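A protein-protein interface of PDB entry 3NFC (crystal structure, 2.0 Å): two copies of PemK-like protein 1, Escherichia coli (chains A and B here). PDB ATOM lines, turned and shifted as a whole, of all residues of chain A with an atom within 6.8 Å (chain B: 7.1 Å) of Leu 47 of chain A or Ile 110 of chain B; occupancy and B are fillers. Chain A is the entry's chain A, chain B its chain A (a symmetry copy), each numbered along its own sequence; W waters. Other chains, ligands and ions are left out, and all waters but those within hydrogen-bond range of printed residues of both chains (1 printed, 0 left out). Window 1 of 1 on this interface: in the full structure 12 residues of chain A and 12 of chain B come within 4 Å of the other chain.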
ATOM      1  N   VAL A  32     -22.739   3.848 -25.899  1.00  0.00           N
ATOM      2  CA  VAL A  32     -23.109   4.155 -24.515  1.00  0.00           C
ATOM      3  C   VAL A  32     -21.918   4.924 -23.873  1.00  0.00           C
ATOM      4  O   VAL A  32     -20.790   4.408 -23.790  1.00  0.00           O
ATOM      5  CB  VAL A  32     -23.452   2.862 -23.687  1.00  0.00           C
ATOM      6  CG1 VAL A  32     -24.042   3.221 -22.292  1.00  0.00           C
ATOM      7  CG2 VAL A  32     -24.398   1.991 -24.490  1.00  0.00           C
ATOM      8  N   VAL A  33     -22.201   6.138 -23.377  1.00  0.00           N
ATOM      9  CA  VAL A  33     -21.176   7.032 -22.764  1.00  0.00           C
ATOM     10  C   VAL A  33     -20.891   6.621 -21.307  1.00  0.00           C
ATOM     11  O   VAL A  33     -21.821   6.448 -20.488  1.00  0.00           O
ATOM     12  CB  VAL A  33     -21.668   8.488 -22.814  1.00  0.00           C
ATOM     13  CG1 VAL A  33     -20.665   9.463 -22.070  1.00  0.00           C
ATOM     14  CG2 VAL A  33     -21.903   8.888 -24.234  1.00  0.00           C
ATOM     15  N   LEU A  34     -19.621   6.422 -21.001  1.00  0.00           N
ATOM     16  CA  LEU A  34     -19.181   5.937 -19.675  1.00  0.00           C
ATOM     17  C   LEU A  34     -18.516   6.984 -18.794  1.00  0.00           C
ATOM     18  O   LEU A  34     -18.555   6.859 -17.549  1.00  0.00           O
ATOM     19  CB  LEU A  34     -18.204   4.752 -19.857  1.00  0.00           C
ATOM     20  CG  LEU A  34     -18.686   3.545 -20.685  1.00  0.00           C
ATOM     21  CD1 LEU A  34     -17.546   2.557 -20.743  1.00  0.00           C
ATOM     22  CD2 LEU A  34     -19.863   2.932 -19.979  1.00  0.00           C
ATOM     23  N   SER A  35     -17.904   8.004 -19.396  1.00  0.00           N
ATOM     24  CA  SER A  35     -17.246   9.060 -18.600  1.00  0.00           C
ATOM     25  C   SER A  35     -18.185  10.233 -18.183  1.00  0.00           C
ATOM     26  O   SER A  35     -19.222  10.462 -18.852  1.00  0.00           O
ATOM     27  CB  SER A  35     -16.038   9.585 -19.381  1.00  0.00           C
ATOM     28  OG  SER A  35     -16.461   9.859 -20.672  1.00  0.00           O
ATOM     29  N   PRO A  36     -17.832  10.970 -17.101  1.00  0.00           N
ATOM     30  CA  PRO A  36     -18.702  12.059 -16.551  1.00  0.00           C
ATOM     31  C   PRO A  36     -18.717  13.342 -17.362  1.00  0.00           C
ATOM     32  O   PRO A  36     -17.716  13.720 -17.970  1.00  0.00           O
ATOM     33  CB  PRO A  36     -18.086  12.364 -15.170  1.00  0.00           C
ATOM     34  CG  PRO A  36     -16.809  11.667 -15.092  1.00  0.00           C
ATOM     35  CD  PRO A  36     -16.576  10.836 -16.320  1.00  0.00           C
ATOM     36  N   TYR A  39     -15.517  15.861 -17.205  1.00  0.00           N
ATOM     37  CA  TYR A  39     -14.475  15.366 -18.133  1.00  0.00           C
ATOM     38  C   TYR A  39     -14.864  15.608 -19.568  1.00  0.00           C
ATOM     39  O   TYR A  39     -14.021  16.096 -20.358  1.00  0.00           O
ATOM     40  CB  TYR A  39     -14.096  13.899 -17.917  1.00  0.00           C
ATOM     41  CG  TYR A  39     -13.072  13.357 -18.912  1.00  0.00           C
ATOM     42  CD1 TYR A  39     -11.699  13.442 -18.667  1.00  0.00           C
ATOM     43  CD2 TYR A  39     -13.492  12.762 -20.090  1.00  0.00           C
ATOM     44  CE1 TYR A  39     -10.760  12.956 -19.603  1.00  0.00           C
ATOM     45  CE2 TYR A  39     -12.622  12.252 -20.990  1.00  0.00           C
ATOM     46  CZ  TYR A  39     -11.245  12.366 -20.782  1.00  0.00           C
ATOM     47  OH  TYR A  39     -10.381  11.840 -21.744  1.00  0.00           O
ATOM     48  N   ASN A  40     -16.126  15.274 -19.933  1.00  0.00           N
ATOM     49  CA  ASN A  40     -16.558  15.366 -21.362  1.00  0.00           C
ATOM     50  C   ASN A  40     -16.516  16.773 -21.941  1.00  0.00           C
ATOM     51  O   ASN A  40     -16.024  17.012 -23.082  1.00  0.00           O
ATOM     52  CB  ASN A  40     -17.967  14.724 -21.593  1.00  0.00           C
ATOM     53  CG  ASN A  40     -18.024  13.303 -21.155  1.00  0.00           C
ATOM     54  OD1 ASN A  40     -16.984  12.609 -21.088  1.00  0.00           O
ATOM     55  ND2 ASN A  40     -19.226  12.823 -20.864  1.00  0.00           N
ATOM     56  N   MET A  45     -13.678  14.989 -25.372  1.00  0.00           N
ATOM     57  CA  MET A  45     -13.611  13.557 -25.624  1.00  0.00           C
ATOM     58  C   MET A  45     -14.552  12.805 -24.644  1.00  0.00           C
ATOM     59  O   MET A  45     -14.972  13.372 -23.591  1.00  0.00           O
ATOM     60  CB  MET A  45     -12.167  13.081 -25.371  1.00  0.00           C
ATOM     61  CG  MET A  45     -11.091  14.008 -25.985  1.00  0.00           C
ATOM     62  SD  MET A  45     -11.031  13.507 -27.688  1.00  0.00           S
ATOM     63  CE  MET A  45     -10.560  14.994 -28.611  1.00  0.00           C
ATOM     64  N   CYS A  46     -14.853  11.553 -24.955  1.00  0.00           N
ATOM     65  CA  CYS A  46     -15.553  10.710 -23.995  1.00  0.00           C
ATOM     66  C   CYS A  46     -15.137   9.250 -24.218  1.00  0.00           C
ATOM     67  O   CYS A  46     -14.723   8.896 -25.344  1.00  0.00           O
ATOM     68  CB  CYS A  46     -17.070  10.939 -24.044  1.00  0.00           C
ATOM     69  SG  CYS A  46     -17.972  10.376 -25.576  1.00  0.00           S
ATOM     70  N   LEU A  47     -15.186   8.439 -23.166  1.00  0.00           N
ATOM     71  CA  LEU A  47     -14.973   6.999 -23.290  1.00  0.00           C
ATOM     72  C   LEU A  47     -16.362   6.396 -23.464  1.00  0.00           C
ATOM     73  O   LEU A  47     -17.319   6.837 -22.775  1.00  0.00           O
ATOM     74  CB  LEU A  47     -14.332   6.476 -21.982  1.00  0.00           C
ATOM     75  CG  LEU A  47     -12.816   6.848 -21.944  1.00  0.00           C
ATOM     76  CD1 LEU A  47     -12.361   6.854 -20.600  1.00  0.00           C
ATOM     77  CD2 LEU A  47     -11.913   5.901 -22.753  1.00  0.00           C
ATOM     78  N   CYS A  48     -16.499   5.427 -24.368  1.00  0.00           N
ATOM     79  CA  CYS A  48     -17.774   4.801 -24.611  1.00  0.00           C
ATOM     80  C   CYS A  48     -17.649   3.425 -25.226  1.00  0.00           C
ATOM     81  O   CYS A  48     -16.558   3.070 -25.736  1.00  0.00           O
ATOM     82  CB  CYS A  48     -18.656   5.730 -25.442  1.00  0.00           C
ATOM     83  SG  CYS A  48     -17.983   6.189 -26.992  1.00  0.00           S
ATOM     84  N   VAL A  49     -18.759   2.663 -25.218  1.00  0.00           N
ATOM     85  CA  VAL A  49     -18.769   1.339 -25.868  1.00  0.00           C
ATOM     86  C   VAL A  49     -19.849   1.243 -26.982  1.00  0.00           C
ATOM     87  O   VAL A  49     -21.002   1.733 -26.793  1.00  0.00           O
ATOM     88  CB  VAL A  49     -19.003   0.170 -24.801  1.00  0.00           C
ATOM     89  CG1 VAL A  49     -17.908   0.165 -23.620  1.00  0.00           C
ATOM     90  CG2 VAL A  49     -20.332   0.263 -24.161  1.00  0.00           C
ATOM     91  N   VAL A  78     -14.448  -0.773 -25.264  1.00  0.00           N
ATOM     92  CA  VAL A  78     -14.419   0.647 -24.871  1.00  0.00           C
ATOM     93  C   VAL A  78     -13.506   1.500 -25.814  1.00  0.00           C
ATOM     94  O   VAL A  78     -12.549   1.021 -26.414  1.00  0.00           O
ATOM     95  CB  VAL A  78     -14.258   0.877 -23.285  1.00  0.00           C
ATOM     96  CG1 VAL A  78     -13.689  -0.374 -22.585  1.00  0.00           C
ATOM     97  CG2 VAL A  78     -13.376   2.111 -22.978  1.00  0.00           C
ATOM     98  N   LYS A  79     -13.863   2.737 -26.066  1.00  0.00           N
ATOM     99  CA  LYS A  79     -12.989   3.568 -26.858  1.00  0.00           C
ATOM    100  C   LYS A  79     -13.109   5.051 -26.445  1.00  0.00           C
ATOM    101  O   LYS A  79     -14.168   5.491 -25.973  1.00  0.00           O
ATOM    102  CB  LYS A  79     -13.277   3.409 -28.332  1.00  0.00           C
ATOM    103  N   SER A  80     -12.011   5.800 -26.661  1.00  0.00           N
ATOM    104  CA  SER A  80     -12.002   7.241 -26.501  1.00  0.00           C
ATOM    105  C   SER A  80     -12.412   7.857 -27.808  1.00  0.00           C
ATOM    106  O   SER A  80     -11.803   7.575 -28.851  1.00  0.00           O
ATOM    107  CB  SER A  80     -10.609   7.746 -26.099  1.00  0.00           C
ATOM    108  OG  SER A  80     -10.624   9.139 -25.832  1.00  0.00           O
ATOM    109  N   ILE A  81     -13.423   8.717 -27.780  1.00  0.00           N
ATOM    110  CA  ILE A  81     -13.908   9.263 -29.004  1.00  0.00           C
ATOM    111  C   ILE A  81     -14.046  10.775 -28.942  1.00  0.00           C
ATOM    112  O   ILE A  81     -14.432  11.338 -27.912  1.00  0.00           O
ATOM    113  CB  ILE A  81     -15.251   8.569 -29.534  1.00  0.00           C
ATOM    114  CG1 ILE A  81     -16.503   9.218 -29.018  1.00  0.00           C
ATOM    115  CG2 ILE A  81     -15.248   6.990 -29.731  1.00  0.00           C
ATOM    116  CD1 ILE A  81     -17.205   9.831 -30.252  1.00  0.00           C
ATOM    117  N   LYS A 103     -20.016  -1.268 -16.731  1.00  0.00           N
ATOM    118  CA  LYS A 103     -18.842  -0.862 -15.946  1.00  0.00           C
ATOM    119  C   LYS A 103     -18.226  -2.046 -15.179  1.00  0.00           C
ATOM    120  O   LYS A 103     -16.963  -2.144 -15.061  1.00  0.00           O
ATOM    121  CB  LYS A 103     -19.179   0.306 -15.031  1.00  0.00           C
ATOM    122  CG  LYS A 103     -19.298   1.590 -15.758  1.00  0.00           C
ATOM    123  CD  LYS A 103     -19.977   2.638 -14.892  1.00  0.00           C
ATOM    124  CE  LYS A 103     -20.029   3.956 -15.708  1.00  0.00           C
ATOM    125  NZ  LYS A 103     -19.549   5.083 -14.832  1.00  0.00           N
ATOM    126  N   ALA A 104     -19.081  -2.948 -14.660  1.00  0.00           N
ATOM    127  CA  ALA A 104     -18.540  -4.075 -13.898  1.00  0.00           C
ATOM    128  C   ALA A 104     -17.770  -5.077 -14.806  1.00  0.00           C
ATOM    129  O   ALA A 104     -16.713  -5.576 -14.424  1.00  0.00           O
ATOM    130  CB  ALA A 104     -19.619  -4.788 -13.035  1.00  0.00           C
ATOM    131  N   ILE A 106     -16.010  -4.337 -17.616  1.00  0.00           N
ATOM    132  CA  ILE A 106     -14.727  -3.660 -17.954  1.00  0.00           C
ATOM    133  C   ILE A 106     -13.737  -3.767 -16.760  1.00  0.00           C
ATOM    134  O   ILE A 106     -12.522  -4.009 -16.915  1.00  0.00           O
ATOM    135  CB  ILE A 106     -14.936  -2.150 -18.246  1.00  0.00           C
ATOM    136  CG1 ILE A 106     -15.697  -1.988 -19.567  1.00  0.00           C
ATOM    137  CG2 ILE A 106     -13.565  -1.388 -18.171  1.00  0.00           C
ATOM    138  CD1 ILE A 106     -16.380  -0.630 -19.759  1.00  0.00           C
ATOM    139  N   ASN A 107     -14.301  -3.568 -15.572  1.00  0.00           N
ATOM    140  CA  ASN A 107     -13.554  -3.659 -14.327  1.00  0.00           C
ATOM    141  C   ASN A 107     -12.955  -5.020 -14.101  1.00  0.00           C
ATOM    142  O   ASN A 107     -11.817  -5.117 -13.665  1.00  0.00           O
ATOM    143  CB  ASN A 107     -14.396  -3.181 -13.120  1.00  0.00           C
ATOM    144  CG  ASN A 107     -13.895  -1.863 -12.605  1.00  0.00           C
ATOM    145  OD1 ASN A 107     -14.299  -0.791 -13.081  1.00  0.00           O
ATOM    146  ND2 ASN A 107     -12.916  -1.930 -11.673  1.00  0.00           N
ATOM    147  N   ILE A 110      -9.993  -5.039 -16.985  1.00  0.00           N
ATOM    148  CA  ILE A 110      -8.842  -4.124 -16.781  1.00  0.00           C
ATOM    149  C   ILE A 110      -8.791  -3.385 -15.454  1.00  0.00           C
ATOM    150  O   ILE A 110      -8.089  -2.381 -15.355  1.00  0.00           O
ATOM    151  CB  ILE A 110      -8.704  -2.964 -17.895  1.00  0.00           C
ATOM    152  CG1 ILE A 110      -9.893  -1.984 -17.835  1.00  0.00           C
ATOM    153  CG2 ILE A 110      -8.489  -3.553 -19.306  1.00  0.00           C
ATOM    154  CD1 ILE A 110      -9.832  -0.829 -18.825  1.00  0.00           C
ATOM    155  N   ALA B  75      -3.356   7.848 -19.790  1.00  0.00           N
ATOM    156  CA  ALA B  75      -4.300   6.827 -19.216  1.00  0.00           C
ATOM    157  C   ALA B  75      -5.773   6.967 -19.645  1.00  0.00           C
ATOM    158  O   ALA B  75      -6.515   5.964 -19.735  1.00  0.00           O
ATOM    159  CB  ALA B  75      -4.204   6.793 -17.612  1.00  0.00           C
ATOM    160  N   ASP B  76      -6.190   8.210 -19.879  1.00  0.00           N
ATOM    161  CA  ASP B  76      -7.550   8.515 -20.292  1.00  0.00           C
ATOM    162  C   ASP B  76      -7.885   8.118 -21.758  1.00  0.00           C
ATOM    163  O   ASP B  76      -9.089   8.064 -22.095  1.00  0.00           O
ATOM    164  CB  ASP B  76      -7.884  10.002 -20.039  1.00  0.00           C
ATOM    165  CG  ASP B  76      -7.097  10.973 -20.930  1.00  0.00           C
ATOM    166  OD1 ASP B  76      -5.895  10.750 -21.203  1.00  0.00           O
ATOM    167  OD2 ASP B  76      -7.673  11.990 -21.327  1.00  0.00           O
ATOM    168  N   GLN B  77      -6.877   7.790 -22.581  1.00  0.00           N
ATOM    169  CA  GLN B  77      -7.069   7.382 -24.004  1.00  0.00           C
ATOM    170  C   GLN B  77      -7.040   5.838 -24.243  1.00  0.00           C
ATOM    171  O   GLN B  77      -6.560   5.349 -25.265  1.00  0.00           O
ATOM    172  CB  GLN B  77      -6.106   8.118 -24.957  1.00  0.00           C
ATOM    173  CG  GLN B  77      -6.252   9.701 -24.878  1.00  0.00           C
ATOM    174  CD  GLN B  77      -5.186  10.518 -25.609  1.00  0.00           C
ATOM    175  OE1 GLN B  77      -4.719  10.159 -26.691  1.00  0.00           O
ATOM    176  NE2 GLN B  77      -4.835  11.663 -25.039  1.00  0.00           N
ATOM    177  N   VAL B  78      -7.532   5.068 -23.272  1.00  0.00           N
ATOM    178  CA  VAL B  78      -7.581   3.610 -23.484  1.00  0.00           C
ATOM    179  C   VAL B  78      -8.232   3.237 -24.858  1.00  0.00           C
ATOM    180  O   VAL B  78      -9.059   3.955 -25.411  1.00  0.00           O
ATOM    181  CB  VAL B  78      -8.067   2.783 -22.191  1.00  0.00           C
ATOM    182  CG1 VAL B  78      -8.828   3.682 -21.195  1.00  0.00           C
ATOM    183  CG2 VAL B  78      -8.939   1.568 -22.589  1.00  0.00           C
ATOM    184  N   LYS B  79      -7.776   2.185 -25.493  1.00  0.00           N
ATOM    185  CA  LYS B  79      -8.422   1.772 -26.715  1.00  0.00           C
ATOM    186  C   LYS B  79      -8.327   0.242 -26.902  1.00  0.00           C
ATOM    187  O   LYS B  79      -7.376  -0.395 -26.427  1.00  0.00           O
ATOM    188  CB  LYS B  79      -7.832   2.484 -27.909  1.00  0.00           C
ATOM    189  N   LYS B 105      -5.993   5.464 -12.381  1.00  0.00           N
ATOM    190  CA  LYS B 105      -6.587   6.657 -13.060  1.00  0.00           C
ATOM    191  C   LYS B 105      -7.820   6.389 -14.007  1.00  0.00           C
ATOM    192  O   LYS B 105      -8.767   7.207 -14.117  1.00  0.00           O
ATOM    193  CB  LYS B 105      -5.478   7.446 -13.737  1.00  0.00           C
ATOM    194  CG  LYS B 105      -4.526   8.163 -12.698  1.00  0.00           C
ATOM    195  CD  LYS B 105      -3.557   9.107 -13.440  1.00  0.00           C
ATOM    196  CE  LYS B 105      -2.458   9.722 -12.530  1.00  0.00           C
ATOM    197  NZ  LYS B 105      -1.780  10.874 -13.235  1.00  0.00           N
ATOM    198  N   ILE B 106      -7.802   5.268 -14.697  1.00  0.00           N
ATOM    199  CA  ILE B 106      -8.951   4.835 -15.540  1.00  0.00           C
ATOM    200  C   ILE B 106     -10.177   4.508 -14.642  1.00  0.00           C
ATOM    201  O   ILE B 106     -11.340   4.846 -14.945  1.00  0.00           O
ATOM    202  CB  ILE B 106      -8.618   3.554 -16.349  1.00  0.00           C
ATOM    203  CG1 ILE B 106      -7.586   3.890 -17.432  1.00  0.00           C
ATOM    204  CG2 ILE B 106      -9.938   2.885 -16.875  1.00  0.00           C
ATOM    205  CD1 ILE B 106      -6.818   2.688 -17.991  1.00  0.00           C
ATOM    206  N   ASN B 107      -9.872   3.834 -13.537  1.00  0.00           N
ATOM    207  CA  ASN B 107     -10.872   3.462 -12.548  1.00  0.00           C
ATOM    208  C   ASN B 107     -11.565   4.649 -11.939  1.00  0.00           C
ATOM    209  O   ASN B 107     -12.774   4.617 -11.754  1.00  0.00           O
ATOM    210  CB  ASN B 107     -10.288   2.511 -11.476  1.00  0.00           C
ATOM    211  CG  ASN B 107     -10.828   1.120 -11.640  1.00  0.00           C
ATOM    212  OD1 ASN B 107     -10.284   0.305 -12.400  1.00  0.00           O
ATOM    213  ND2 ASN B 107     -11.985   0.859 -10.990  1.00  0.00           N
ATOM    214  N   VAL B 108     -10.815   5.709 -11.657  1.00  0.00           N
ATOM    215  CA  VAL B 108     -11.434   6.951 -11.191  1.00  0.00           C
ATOM    216  C   VAL B 108     -12.381   7.524 -12.293  1.00  0.00           C
ATOM    217  O   VAL B 108     -13.477   7.991 -12.014  1.00  0.00           O
ATOM    218  CB  VAL B 108     -10.362   7.960 -10.753  1.00  0.00           C
ATOM    219  CG1 VAL B 108     -10.937   9.387 -10.624  1.00  0.00           C
ATOM    220  CG2 VAL B 108      -9.636   7.475  -9.448  1.00  0.00           C
ATOM    221  N   LEU B 109     -11.931   7.490 -13.535  1.00  0.00           N
ATOM    222  CA  LEU B 109     -12.672   8.081 -14.631  1.00  0.00           C
ATOM    223  C   LEU B 109     -13.946   7.265 -15.036  1.00  0.00           C
ATOM    224  O   LEU B 109     -15.010   7.868 -15.215  1.00  0.00           O
ATOM    225  CB  LEU B 109     -11.734   8.343 -15.826  1.00  0.00           C
ATOM    226  CG  LEU B 109     -12.321   9.026 -17.078  1.00  0.00           C
ATOM    227  CD1 LEU B 109     -12.760  10.436 -16.778  1.00  0.00           C
ATOM    228  CD2 LEU B 109     -11.258   9.082 -18.162  1.00  0.00           C
ATOM    229  N   ILE B 110     -13.839   5.931 -15.144  1.00  0.00           N
ATOM    230  CA  ILE B 110     -14.966   5.062 -15.568  1.00  0.00           C
ATOM    231  C   ILE B 110     -15.267   3.864 -14.682  1.00  0.00           C
ATOM    232  O   ILE B 110     -15.928   2.934 -15.138  1.00  0.00           O
ATOM    233  CB  ILE B 110     -14.811   4.440 -17.049  1.00  0.00           C
ATOM    234  CG1 ILE B 110     -13.620   3.463 -17.126  1.00  0.00           C
ATOM    235  CG2 ILE B 110     -14.745   5.545 -18.125  1.00  0.00           C
ATOM    236  CD1 ILE B 110     -13.416   2.794 -18.478  1.00  0.00           C
ATOM    237  N   GLY B 111     -14.810   3.864 -13.432  1.00  0.00           N
ATOM    238  CA  GLY B 111     -15.013   2.718 -12.532  1.00  0.00           C
ATOM    239  C   GLY B 111     -16.373   2.753 -11.888  1.00  0.00           C
ATOM    240  O   GLY B 111     -16.925   1.712 -11.527  1.00  0.00           O
ATOM    241  OXT GLY B 111     -16.972   3.821 -11.722  1.00  0.00           O
HETATM  242  O   HOH W   1     -11.331   9.836 -23.417  1.00  0.00           O
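N of Leu 34 of chain A sits at hydrogen-bond distance from O of Leu 47 of chain A (2.9 Å). O of Leu 34 of chain A lies within hydrogen-bond range of NZ of Lys 103 of chain A (3.4 Å). The side-chain hydroxyl (OG) of Ser 35 of chain A is in hydrogen-bond range of the backbone NH (N) of Leu 47 of chain A (3.1 Å). The backbone carbonyl oxygen (O) of Pro 36 of chain A sits close to the side-chain amide nitrogen (ND2) of Asn 40 of chain A, 3.4 Å away.
Hydrophobic or aromatic side chains of chain B within 4 Å of the printed part of chain A: Leu 109 and Ile 110. Printed residues of chain A that touch a printed residue of chain B: Leu 34, Pro 36, Tyr 39, Leu 47, Ser 80, Lys 103 and Asn 107. Hydrophobic or aromatic side chains of chain A that line the printed part of chain B: Leu 34, Pro 36, Tyr 39 and Leu 47. Along chain A the printed residues that touch a printed residue of chain B span positions 34 to 107.
The side-chain hydroxyl (OH) of Tyr 39 of chain A sits at hydrogen-bond distance from the side-chain carboxylate (OD2) of Asp 76 of chain B (2.7 Å). The side-chain amide nitrogen (ND2) of Asn 107 of chain A lies close to the side-chain amide nitrogen (ND2) of Asn 107 of chain B.
Asn 107 of chain A touches its own counterpart, Asn 107 of chain B. Positions printed for both chains: 78, 79, 106, 107 and 110.
Of the printed residues of chain B, Leu 47 of chain A touches Asp 76 (3.6 Å), Leu 109 (3.5 Å) and Ile 110 (3.7 Å). Of the printed residues of chain B, Ser 80 of chain A touches Val 78. Printed residues of chain A within 4 Å of Asp 76 of chain B: Tyr 39 (2.7 Å) and Leu 47 (3.6 Å). Printed residues of chain B within 4 Å of Asn 107 of chain A: Asn 107 and Gly 111. Printed residues of chain A within 4 Å of Asn 107 of chain B: Asn 107 (3.0 Å). Printed residues of chain A within 4 Å of Val 78 of chain B: Ser 80. Val 32 of chain A touches none of the printed residues of chain B. The nearest residue of chain B that does not touch Leu 47 of chain A is Val 78 of chain B (4.1 Å). The nearest printed residue of chain A that does not touch Ile 110 of chain B is Ile 106 of chain A (4.2 Å).
Among the printed residues, merely in contact across the chains: Leu 47 of chain A with Leu 109 of chain B (3.5 Å), Pro 36 of chain A with Leu 109 of chain B (3.5 Å), Leu 47 of chain A with Asp 76 of chain B (3.6 Å), Asn 107 of chain A with Gly 111 of chain B (3.6 Å), Tyr 39 of chain A with Leu 109 of chain B (3.6 Å), Leu 47 of chain A with Ile 110 of chain B (3.7 Å), Lys 103 of chain A with Ile 110 of chain B (3.7 Å), Ser 80 of chain A with Val 78 of chain B (3.7 Å) and Leu 34 of chain A with Ile 110 of chain B (3.9 Å).
Water W1 lies within hydrogen-bond range of OG of Ser 80 of chain A (2.6 Å), OH of Tyr 39 of chain A (2.8 Å) and O of Asp 76 of chain B (3.1 Å).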
